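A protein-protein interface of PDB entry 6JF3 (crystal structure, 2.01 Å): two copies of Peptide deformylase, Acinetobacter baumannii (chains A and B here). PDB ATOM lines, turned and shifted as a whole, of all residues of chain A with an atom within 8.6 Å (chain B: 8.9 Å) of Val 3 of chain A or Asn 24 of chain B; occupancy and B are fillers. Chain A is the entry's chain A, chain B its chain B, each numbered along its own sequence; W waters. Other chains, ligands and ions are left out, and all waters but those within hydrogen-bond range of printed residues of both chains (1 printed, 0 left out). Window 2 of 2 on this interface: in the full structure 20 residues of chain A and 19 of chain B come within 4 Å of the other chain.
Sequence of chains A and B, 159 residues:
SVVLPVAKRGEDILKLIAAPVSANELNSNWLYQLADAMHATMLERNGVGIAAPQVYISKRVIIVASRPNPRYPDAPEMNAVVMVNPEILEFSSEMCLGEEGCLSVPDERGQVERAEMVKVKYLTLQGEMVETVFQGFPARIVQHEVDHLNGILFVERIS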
ATOM      1  N   SER A   1       8.684 -23.625 -24.266  1.00  0.00           N
ATOM      2  CA  SER A   1       7.256 -23.697 -23.812  1.00  0.00           C
ATOM      3  C   SER A   1       7.131 -23.334 -22.354  1.00  0.00           C
ATOM      4  O   SER A   1       8.090 -23.400 -21.617  1.00  0.00           O
ATOM      5  CB  SER A   1       6.678 -25.096 -24.012  1.00  0.00           C
ATOM      6  OG  SER A   1       6.525 -25.376 -25.389  1.00  0.00           O
ATOM      7  N   VAL A   2       5.929 -22.995 -21.930  1.00  0.00           N
ATOM      8  CA  VAL A   2       5.688 -22.570 -20.550  1.00  0.00           C
ATOM      9  C   VAL A   2       5.096 -23.706 -19.724  1.00  0.00           C
ATOM     10  O   VAL A   2       4.066 -24.326 -20.096  1.00  0.00           O
ATOM     11  CB  VAL A   2       4.746 -21.365 -20.549  1.00  0.00           C
ATOM     12  CG1 VAL A   2       4.327 -20.986 -19.149  1.00  0.00           C
ATOM     13  CG2 VAL A   2       5.446 -20.206 -21.206  1.00  0.00           C
ATOM     14  N   VAL A   3       5.734 -23.964 -18.592  1.00  0.00           N
ATOM     15  CA  VAL A   3       5.154 -24.806 -17.567  1.00  0.00           C
ATOM     16  C   VAL A   3       4.306 -23.941 -16.635  1.00  0.00           C
ATOM     17  O   VAL A   3       4.820 -22.999 -16.069  1.00  0.00           O
ATOM     18  CB  VAL A   3       6.201 -25.529 -16.763  1.00  0.00           C
ATOM     19  CG1 VAL A   3       5.534 -26.293 -15.619  1.00  0.00           C
ATOM     20  CG2 VAL A   3       6.951 -26.503 -17.660  1.00  0.00           C
ATOM     21  N   LEU A   4       3.017 -24.295 -16.485  1.00  0.00           N
ATOM     22  CA  LEU A   4       2.037 -23.494 -15.753  1.00  0.00           C
ATOM     23  C   LEU A   4       1.832 -24.047 -14.335  1.00  0.00           C
ATOM     24  O   LEU A   4       2.028 -25.239 -14.098  1.00  0.00           O
ATOM     25  CB  LEU A   4       0.685 -23.497 -16.494  1.00  0.00           C
ATOM     26  CG  LEU A   4       0.579 -22.881 -17.891  1.00  0.00           C
ATOM     27  CD1 LEU A   4      -0.804 -23.102 -18.527  1.00  0.00           C
ATOM     28  CD2 LEU A   4       0.872 -21.392 -17.825  1.00  0.00           C
ATOM     29  N   PRO A   5       1.431 -23.183 -13.382  1.00  0.00           N
ATOM     30  CA  PRO A   5       1.073 -23.709 -12.059  1.00  0.00           C
ATOM     31  C   PRO A   5      -0.246 -24.502 -12.104  1.00  0.00           C
ATOM     32  O   PRO A   5      -1.158 -24.156 -12.891  1.00  0.00           O
ATOM     33  CB  PRO A   5       0.878 -22.436 -11.216  1.00  0.00           C
ATOM     34  CG  PRO A   5       0.473 -21.415 -12.195  1.00  0.00           C
ATOM     35  CD  PRO A   5       1.252 -21.723 -13.447  1.00  0.00           C
ATOM     36  N   VAL A   6      -0.343 -25.510 -11.239  1.00  0.00           N
ATOM     37  CA  VAL A   6      -1.451 -26.453 -11.247  1.00  0.00           C
ATOM     38  C   VAL A   6      -2.253 -26.342  -9.965  1.00  0.00           C
ATOM     39  O   VAL A   6      -1.664 -26.296  -8.900  1.00  0.00           O
ATOM     40  CB  VAL A   6      -0.945 -27.914 -11.436  1.00  0.00           C
ATOM     41  CG1 VAL A   6      -2.061 -28.926 -11.185  1.00  0.00           C
ATOM     42  CG2 VAL A   6      -0.373 -28.119 -12.835  1.00  0.00           C
ATOM     43  N   ASP A  36      -0.656 -25.316 -26.095  1.00  0.00           N
ATOM     44  CA  ASP A  36       0.787 -25.568 -25.932  1.00  0.00           C
ATOM     45  C   ASP A  36       1.312 -25.595 -24.460  1.00  0.00           C
ATOM     46  O   ASP A  36       2.088 -26.482 -24.066  1.00  0.00           O
ATOM     47  CB  ASP A  36       1.571 -24.520 -26.685  1.00  0.00           C
ATOM     48  CG  ASP A  36       3.032 -24.911 -26.837  1.00  0.00           C
ATOM     49  OD1 ASP A  36       3.328 -25.658 -27.799  1.00  0.00           O
ATOM     50  OD2 ASP A  36       3.881 -24.484 -25.998  1.00  0.00           O
ATOM     51  N   ALA A  37       0.883 -24.612 -23.682  1.00  0.00           N
ATOM     52  CA  ALA A  37       1.222 -24.501 -22.227  1.00  0.00           C
ATOM     53  C   ALA A  37       0.640 -25.643 -21.427  1.00  0.00           C
ATOM     54  O   ALA A  37       1.341 -26.203 -20.557  1.00  0.00           O
ATOM     55  CB  ALA A  37       0.743 -23.153 -21.654  1.00  0.00           C
ATOM     56  N   MET A  38      -0.615 -26.025 -21.737  1.00  0.00           N
ATOM     57  CA  MET A  38      -1.197 -27.191 -21.100  1.00  0.00           C
ATOM     58  C   MET A  38      -0.380 -28.441 -21.424  1.00  0.00           C
ATOM     59  O   MET A  38      -0.123 -29.279 -20.531  1.00  0.00           O
ATOM     60  CB  MET A  38      -2.650 -27.418 -21.493  1.00  0.00           C
ATOM     61  CG  MET A  38      -3.598 -26.387 -20.911  1.00  0.00           C
ATOM     62  SD  MET A  38      -5.242 -26.617 -21.698  1.00  0.00           S
ATOM     63  CE  MET A  38      -5.607 -28.305 -21.214  1.00  0.00           C
ATOM     64  N   HIS A  39       0.029 -28.552 -22.693  1.00  0.00           N
ATOM     65  CA  HIS A  39       0.790 -29.687 -23.129  1.00  0.00           C
ATOM     66  C   HIS A  39       2.153 -29.765 -22.406  1.00  0.00           C
ATOM     67  O   HIS A  39       2.459 -30.779 -21.806  1.00  0.00           O
ATOM     68  CB  HIS A  39       0.965 -29.738 -24.664  1.00  0.00           C
ATOM     69  CG  HIS A  39       1.527 -31.055 -25.114  1.00  0.00           C
ATOM     70  ND1 HIS A  39       0.990 -32.258 -24.701  1.00  0.00           N
ATOM     71  CD2 HIS A  39       2.620 -31.371 -25.845  1.00  0.00           C
ATOM     72  CE1 HIS A  39       1.705 -33.260 -25.185  1.00  0.00           C
ATOM     73  NE2 HIS A  39       2.692 -32.751 -25.897  1.00  0.00           N
ATOM     74  N   ALA A  40       2.948 -28.704 -22.465  1.00  0.00           N
ATOM     75  CA  ALA A  40       4.193 -28.636 -21.685  1.00  0.00           C
ATOM     76  C   ALA A  40       4.052 -29.004 -20.207  1.00  0.00           C
ATOM     77  O   ALA A  40       4.867 -29.710 -19.668  1.00  0.00           O
ATOM     78  CB  ALA A  40       4.802 -27.239 -21.795  1.00  0.00           C
ATOM     79  N   THR A  41       3.012 -28.496 -19.563  1.00  0.00           N
ATOM     80  CA  THR A  41       2.750 -28.731 -18.146  1.00  0.00           C
ATOM     81  C   THR A  41       2.443 -30.190 -17.849  1.00  0.00           C
ATOM     82  O   THR A  41       2.885 -30.741 -16.824  1.00  0.00           O
ATOM     83  CB  THR A  41       1.550 -27.818 -17.691  1.00  0.00           C
ATOM     84  OG1 THR A  41       1.859 -26.472 -18.005  1.00  0.00           O
ATOM     85  CG2 THR A  41       1.254 -27.909 -16.251  1.00  0.00           C
ATOM     86  N   MET A  42       1.627 -30.806 -18.698  1.00  0.00           N
ATOM     87  CA  MET A  42       1.315 -32.248 -18.571  1.00  0.00           C
ATOM     88  C   MET A  42       2.630 -33.076 -18.691  1.00  0.00           C
ATOM     89  O   MET A  42       2.882 -33.905 -17.851  1.00  0.00           O
ATOM     90  CB  MET A  42       0.301 -32.662 -19.664  1.00  0.00           C
ATOM     91  CG  MET A  42      -0.179 -34.112 -19.642  1.00  0.00           C
ATOM     92  SD  MET A  42      -0.924 -34.626 -21.220  1.00  0.00           S
ATOM     93  CE  MET A  42       0.607 -34.704 -22.167  1.00  0.00           C
ATOM     94  N   LEU A  43       3.451 -32.823 -19.725  1.00  0.00           N
ATOM     95  CA  LEU A  43       4.706 -33.555 -19.934  1.00  0.00           C
ATOM     96  C   LEU A  43       5.599 -33.389 -18.748  1.00  0.00           C
ATOM     97  O   LEU A  43       6.016 -34.344 -18.176  1.00  0.00           O
ATOM     98  CB  LEU A  43       5.446 -33.065 -21.198  1.00  0.00           C
ATOM     99  CG  LEU A  43       4.673 -33.269 -22.517  1.00  0.00           C
ATOM    100  CD1 LEU A  43       5.472 -32.756 -23.698  1.00  0.00           C
ATOM    101  CD2 LEU A  43       4.301 -34.758 -22.665  1.00  0.00           C
ATOM    102  N   GLU A  44       5.790 -32.168 -18.309  1.00  0.00           N
ATOM    103  CA  GLU A  44       6.673 -31.894 -17.163  1.00  0.00           C
ATOM    104  C   GLU A  44       6.171 -32.460 -15.835  1.00  0.00           C
ATOM    105  O   GLU A  44       6.961 -32.640 -14.927  1.00  0.00           O
ATOM    106  CB  GLU A  44       6.861 -30.369 -17.026  1.00  0.00           C
ATOM    107  CG  GLU A  44       7.937 -29.887 -16.066  1.00  0.00           C
ATOM    108  CD  GLU A  44       9.374 -29.853 -16.618  1.00  0.00           C
ATOM    109  OE1 GLU A  44       9.573 -30.272 -17.783  1.00  0.00           O
ATOM    110  OE2 GLU A  44      10.312 -29.392 -15.885  1.00  0.00           O
ATOM    111  N   ARG A  45       4.867 -32.706 -15.703  1.00  0.00           N
ATOM    112  CA  ARG A  45       4.316 -33.341 -14.500  1.00  0.00           C
ATOM    113  C   ARG A  45       4.119 -34.849 -14.672  1.00  0.00           C
ATOM    114  O   ARG A  45       3.502 -35.499 -13.811  1.00  0.00           O
ATOM    115  CB  ARG A  45       2.983 -32.703 -14.098  1.00  0.00           C
ATOM    116  CG  ARG A  45       3.050 -31.204 -13.777  1.00  0.00           C
ATOM    117  CD  ARG A  45       3.299 -30.866 -12.302  1.00  0.00           C
ATOM    118  NE  ARG A  45       2.321 -31.473 -11.373  1.00  0.00           N
ATOM    119  CZ  ARG A  45       1.857 -30.922 -10.242  1.00  0.00           C
ATOM    120  NH1 ARG A  45       0.980 -31.604  -9.499  1.00  0.00           N
ATOM    121  NH2 ARG A  45       2.234 -29.711  -9.839  1.00  0.00           N
ATOM    122  N   VAL A  55      -5.036 -25.823 -14.748  1.00  0.00           N
ATOM    123  CA  VAL A  55      -4.115 -24.689 -14.862  1.00  0.00           C
ATOM    124  C   VAL A  55      -4.862 -23.346 -14.734  1.00  0.00           C
ATOM    125  O   VAL A  55      -4.410 -22.294 -15.261  1.00  0.00           O
ATOM    126  CB  VAL A  55      -3.259 -24.765 -16.123  1.00  0.00           C
ATOM    127  CG1 VAL A  55      -2.401 -25.989 -16.061  1.00  0.00           C
ATOM    128  CG2 VAL A  55      -4.112 -24.772 -17.391  1.00  0.00           C
ATOM    129  N   PRO B  20      -1.976 -16.404  -8.370  1.00  0.00           N
ATOM    130  CA  PRO B  20      -0.895 -15.566  -8.917  1.00  0.00           C
ATOM    131  C   PRO B  20      -0.320 -16.108 -10.223  1.00  0.00           C
ATOM    132  O   PRO B  20      -0.296 -17.295 -10.414  1.00  0.00           O
ATOM    133  CB  PRO B  20       0.183 -15.647  -7.834  1.00  0.00           C
ATOM    134  CG  PRO B  20      -0.570 -15.902  -6.591  1.00  0.00           C
ATOM    135  CD  PRO B  20      -1.647 -16.875  -7.007  1.00  0.00           C
ATOM    136  N   VAL B  21       0.080 -15.229 -11.124  1.00  0.00           N
ATOM    137  CA  VAL B  21       0.854 -15.597 -12.293  1.00  0.00           C
ATOM    138  C   VAL B  21       2.240 -16.020 -11.821  1.00  0.00           C
ATOM    139  O   VAL B  21       2.834 -15.342 -11.016  1.00  0.00           O
ATOM    140  CB  VAL B  21       0.940 -14.397 -13.280  1.00  0.00           C
ATOM    141  CG1 VAL B  21       1.896 -14.674 -14.461  1.00  0.00           C
ATOM    142  CG2 VAL B  21      -0.447 -13.997 -13.773  1.00  0.00           C
ATOM    143  N   SER B  22       2.741 -17.118 -12.359  1.00  0.00           N
ATOM    144  CA  SER B  22       4.003 -17.659 -11.975  1.00  0.00           C
ATOM    145  C   SER B  22       5.164 -17.000 -12.764  1.00  0.00           C
ATOM    146  O   SER B  22       4.959 -16.369 -13.826  1.00  0.00           O
ATOM    147  CB  SER B  22       3.978 -19.143 -12.250  1.00  0.00           C
ATOM    148  OG  SER B  22       4.105 -19.348 -13.635  1.00  0.00           O
ATOM    149  N   ALA B  23       6.381 -17.208 -12.264  1.00  0.00           N
ATOM    150  CA  ALA B  23       7.630 -16.760 -12.929  1.00  0.00           C
ATOM    151  C   ALA B  23       7.795 -17.282 -14.370  1.00  0.00           C
ATOM    152  O   ALA B  23       8.167 -16.551 -15.248  1.00  0.00           O
ATOM    153  CB  ALA B  23       8.820 -17.172 -12.104  1.00  0.00           C
ATOM    154  N   ASN B  24       7.365 -18.506 -14.614  1.00  0.00           N
ATOM    155  CA  ASN B  24       7.544 -19.138 -15.924  1.00  0.00           C
ATOM    156  C   ASN B  24       6.722 -18.468 -16.997  1.00  0.00           C
ATOM    157  O   ASN B  24       7.060 -18.554 -18.172  1.00  0.00           O
ATOM    158  CB  ASN B  24       7.129 -20.593 -15.920  1.00  0.00           C
ATOM    159  CG  ASN B  24       7.761 -21.366 -14.851  1.00  0.00           C
ATOM    160  OD1 ASN B  24       8.482 -22.310 -15.108  1.00  0.00           O
ATOM    161  ND2 ASN B  24       7.502 -20.977 -13.629  1.00  0.00           N
ATOM    162  N   GLU B  25       5.624 -17.842 -16.594  1.00  0.00           N
ATOM    163  CA  GLU B  25       4.717 -17.200 -17.531  1.00  0.00           C
ATOM    164  C   GLU B  25       5.177 -15.830 -17.901  1.00  0.00           C
ATOM    165  O   GLU B  25       4.725 -15.287 -18.954  1.00  0.00           O
ATOM    166  CB  GLU B  25       3.315 -17.128 -16.938  1.00  0.00           C
ATOM    167  CG  GLU B  25       2.736 -18.483 -16.539  1.00  0.00           C
ATOM    168  CD  GLU B  25       1.464 -18.355 -15.699  1.00  0.00           C
ATOM    169  OE1 GLU B  25       1.486 -18.675 -14.477  1.00  0.00           O
ATOM    170  OE2 GLU B  25       0.418 -17.929 -16.265  1.00  0.00           O
ATOM    171  N   LEU B  26       6.057 -15.229 -17.078  1.00  0.00           N
ATOM    172  CA  LEU B  26       6.518 -13.853 -17.353  1.00  0.00           C
ATOM    173  C   LEU B  26       7.278 -13.876 -18.668  1.00  0.00           C
ATOM    174  O   LEU B  26       7.939 -14.858 -19.002  1.00  0.00           O
ATOM    175  CB  LEU B  26       7.339 -13.239 -16.206  1.00  0.00           C
ATOM    176  CG  LEU B  26       6.588 -13.100 -14.858  1.00  0.00           C
ATOM    177  CD1 LEU B  26       7.534 -12.759 -13.698  1.00  0.00           C
ATOM    178  CD2 LEU B  26       5.463 -12.079 -14.972  1.00  0.00           C
ATOM    179  N   ASN B  27       7.036 -12.853 -19.468  1.00  0.00           N
ATOM    180  CA  ASN B  27       7.690 -12.681 -20.775  1.00  0.00           C
ATOM    181  C   ASN B  27       7.443 -13.893 -21.695  1.00  0.00           C
ATOM    182  O   ASN B  27       8.337 -14.287 -22.434  1.00  0.00           O
ATOM    183  CB  ASN B  27       9.206 -12.396 -20.546  1.00  0.00           C
ATOM    184  CG  ASN B  27       9.877 -11.675 -21.720  1.00  0.00           C
ATOM    185  OD1 ASN B  27      10.978 -12.044 -22.070  1.00  0.00           O
ATOM    186  ND2 ASN B  27       9.220 -10.683 -22.334  1.00  0.00           N
ATOM    187  N   SER B  28       6.253 -14.516 -21.626  1.00  0.00           N
ATOM    188  CA  SER B  28       5.957 -15.672 -22.501  1.00  0.00           C
ATOM    189  C   SER B  28       4.982 -15.255 -23.560  1.00  0.00           C
ATOM    190  O   SER B  28       4.268 -14.247 -23.386  1.00  0.00           O
ATOM    191  CB  SER B  28       5.421 -16.872 -21.723  1.00  0.00           C
ATOM    192  OG  SER B  28       4.111 -16.641 -21.200  1.00  0.00           O
ATOM    193  N   ASN B  29       4.948 -15.998 -24.665  1.00  0.00           N
ATOM    194  CA  ASN B  29       3.895 -15.818 -25.681  1.00  0.00           C
ATOM    195  C   ASN B  29       2.530 -16.115 -25.092  1.00  0.00           C
ATOM    196  O   ASN B  29       1.558 -15.461 -25.435  1.00  0.00           O
ATOM    197  CB  ASN B  29       4.106 -16.739 -26.875  1.00  0.00           C
ATOM    198  CG  ASN B  29       5.335 -16.371 -27.646  1.00  0.00           C
ATOM    199  OD1 ASN B  29       5.486 -15.215 -28.053  1.00  0.00           O
ATOM    200  ND2 ASN B  29       6.247 -17.337 -27.826  1.00  0.00           N
ATOM    201  N   TRP B  30       2.493 -17.099 -24.190  1.00  0.00           N
ATOM    202  CA  TRP B  30       1.309 -17.437 -23.433  1.00  0.00           C
ATOM    203  C   TRP B  30       0.695 -16.162 -22.824  1.00  0.00           C
ATOM    204  O   TRP B  30      -0.440 -15.775 -23.149  1.00  0.00           O
ATOM    205  CB  TRP B  30       1.672 -18.498 -22.379  1.00  0.00           C
ATOM    206  CG  TRP B  30       0.787 -18.470 -21.203  1.00  0.00           C
ATOM    207  CD1 TRP B  30       1.144 -18.196 -19.907  1.00  0.00           C
ATOM    208  CD2 TRP B  30      -0.617 -18.664 -21.206  1.00  0.00           C
ATOM    209  NE1 TRP B  30       0.031 -18.206 -19.101  1.00  0.00           N
ATOM    210  CE2 TRP B  30      -1.066 -18.506 -19.865  1.00  0.00           C
ATOM    211  CE3 TRP B  30      -1.554 -18.938 -22.214  1.00  0.00           C
ATOM    212  CZ2 TRP B  30      -2.422 -18.597 -19.502  1.00  0.00           C
ATOM    213  CZ3 TRP B  30      -2.919 -19.049 -21.858  1.00  0.00           C
ATOM    214  CH2 TRP B  30      -3.335 -18.877 -20.506  1.00  0.00           C
ATOM    215  N   LEU B  31       1.483 -15.470 -22.002  1.00  0.00           N
ATOM    216  CA  LEU B  31       0.987 -14.316 -21.254  1.00  0.00           C
ATOM    217  C   LEU B  31       0.712 -13.119 -22.168  1.00  0.00           C
ATOM    218  O   LEU B  31      -0.240 -12.382 -21.945  1.00  0.00           O
ATOM    219  CB  LEU B  31       1.988 -13.951 -20.150  1.00  0.00           C
ATOM    220  CG  LEU B  31       1.470 -12.969 -19.096  1.00  0.00           C
ATOM    221  CD1 LEU B  31       0.342 -13.615 -18.306  1.00  0.00           C
ATOM    222  CD2 LEU B  31       2.591 -12.525 -18.179  1.00  0.00           C
ATOM    223  N   LYS B  59      -6.670 -16.016 -12.833  1.00  0.00           N
ATOM    224  CA  LYS B  59      -5.304 -15.547 -12.703  1.00  0.00           C
ATOM    225  C   LYS B  59      -5.305 -14.053 -12.424  1.00  0.00           C
ATOM    226  O   LYS B  59      -6.204 -13.305 -12.861  1.00  0.00           O
ATOM    227  CB  LYS B  59      -4.540 -15.840 -13.976  1.00  0.00           C
ATOM    228  CG  LYS B  59      -4.305 -17.329 -14.155  1.00  0.00           C
ATOM    229  CD  LYS B  59      -3.040 -17.571 -14.936  1.00  0.00           C
ATOM    230  CE  LYS B  59      -2.577 -19.017 -14.858  1.00  0.00           C
ATOM    231  NZ  LYS B  59      -1.408 -19.172 -13.971  1.00  0.00           N
ATOM    232  N   LEU B 125       4.310  -7.364 -18.048  1.00  0.00           N
ATOM    233  CA  LEU B 125       4.352  -8.640 -18.803  1.00  0.00           C
ATOM    234  C   LEU B 125       5.762  -9.247 -18.915  1.00  0.00           C
ATOM    235  O   LEU B 125       5.887 -10.454 -19.011  1.00  0.00           O
ATOM    236  CB  LEU B 125       3.723  -8.482 -20.204  1.00  0.00           C
ATOM    237  CG  LEU B 125       2.216  -8.208 -20.211  1.00  0.00           C
ATOM    238  CD1 LEU B 125       1.737  -7.685 -21.565  1.00  0.00           C
ATOM    239  CD2 LEU B 125       1.412  -9.450 -19.831  1.00  0.00           C
HETATM  240  O   HOH W   1      -1.721 -21.951 -14.428  1.00  0.00           O
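OE1 of Glu 25 of chain B lies within salt-bridge range of NZ of Lys 59 of chain B, 3.0 Å away.
OG of Ser 22 of chain B lies within hydrogen-bond range of OE1 of Glu 25 of chain B (2.8 Å).
The side-chain carboxylate (OE2) of Glu 25 of chain B lies within hydrogen-bond range of the indole nitrogen (NE1) of Trp 30 of chain B, 2.9 Å away.
The backbone NH (N) of Trp 30 of chain B lies close to the side-chain hydroxyl (OG) of Ser 28 of chain B.
OG of Ser 28 of chain B is in hydrogen-bond range of N of Leu 31 of chain B (3.0 Å).
The backbone carbonyl oxygen (O) of Glu 25 of chain B lies within hydrogen-bond range of the side-chain hydroxyl (OG) of Ser 28 of chain B (2.7 Å).
Among the printed residues, merely in contact across the chains: Pro 5 of chain A with Glu 25 of chain B (3.2 Å), Val 3 of chain A with Asn 24 of chain B (3.3 Å), Val 2 of chain A with Ser 28 of chain B (3.4 Å), Pro 5 of chain A with Lys 59 of chain B (3.4 Å), Leu 4 of chain A with Trp 30 of chain B (3.5 Å), Leu 4 of chain A with Glu 25 of chain B (3.7 Å), Pro 5 of chain A with Ser 22 of chain B (3.7 Å), Val 55 of chain A with Lys 59 of chain B (3.8 Å), Val 2 of chain A with Asn 24 of chain B (3.8 Å) and Val 2 of chain A with Glu 25 of chain B (3.95 Å).
No position is printed for both chains.
Water W1 lies within hydrogen-bond range of the backbone carbonyl oxygen of Pro 5 of chain A (2.7 Å), the side-chain amino group of Lys 59 of chain B (2.8 Å) and the backbone carbonyl oxygen of Val 55 of chain A (2.8 Å).
Printed residues of chain A that touch a printed residue of chain B: Val 2, Val 3, Leu 4, Pro 5 and Val 55.
Hydrophobic or aromatic side chains of chain A that line the printed part of chain B: Val 2, Leu 4 and Pro 5.
Along chain A the printed residues that touch a printed residue of chain B span positions 2 to 55.
Of the 14 printed residues of chain B, 6 touch a printed residue of chain A.
Hydrophobic or aromatic side chains of chain B within 4 Å of the printed part of chain A: Trp 30.
Among the printed residues, 10 pairs touch across the chains.
Val 3 of chain A touches just one residue of chain B: Asn 24.
Of the printed residues of chain A, Asn 24 of chain B touches Val 2 (3.8 Å) and Val 3 (3.3 Å).
Val 2 of chain A touches just these residues of chain B: Asn 24 (3.8 Å), Glu 25 (3.95 Å) and Ser 28 (3.4 Å).
No residue of chain A comes within 4 Å of Ala 23 of chain B.
Printed residues of chain A within 4 Å of Ser 28 of chain B: Val 2.
Of the printed residues of chain B, Pro 5 of chain A touches Ser 22 (3.7 Å), Glu 25 (3.2 Å) and Lys 59 (3.4 Å).
The nearest residue of chain B that does not touch Val 3 of chain A is Ser 22 of chain B (4.4 Å).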
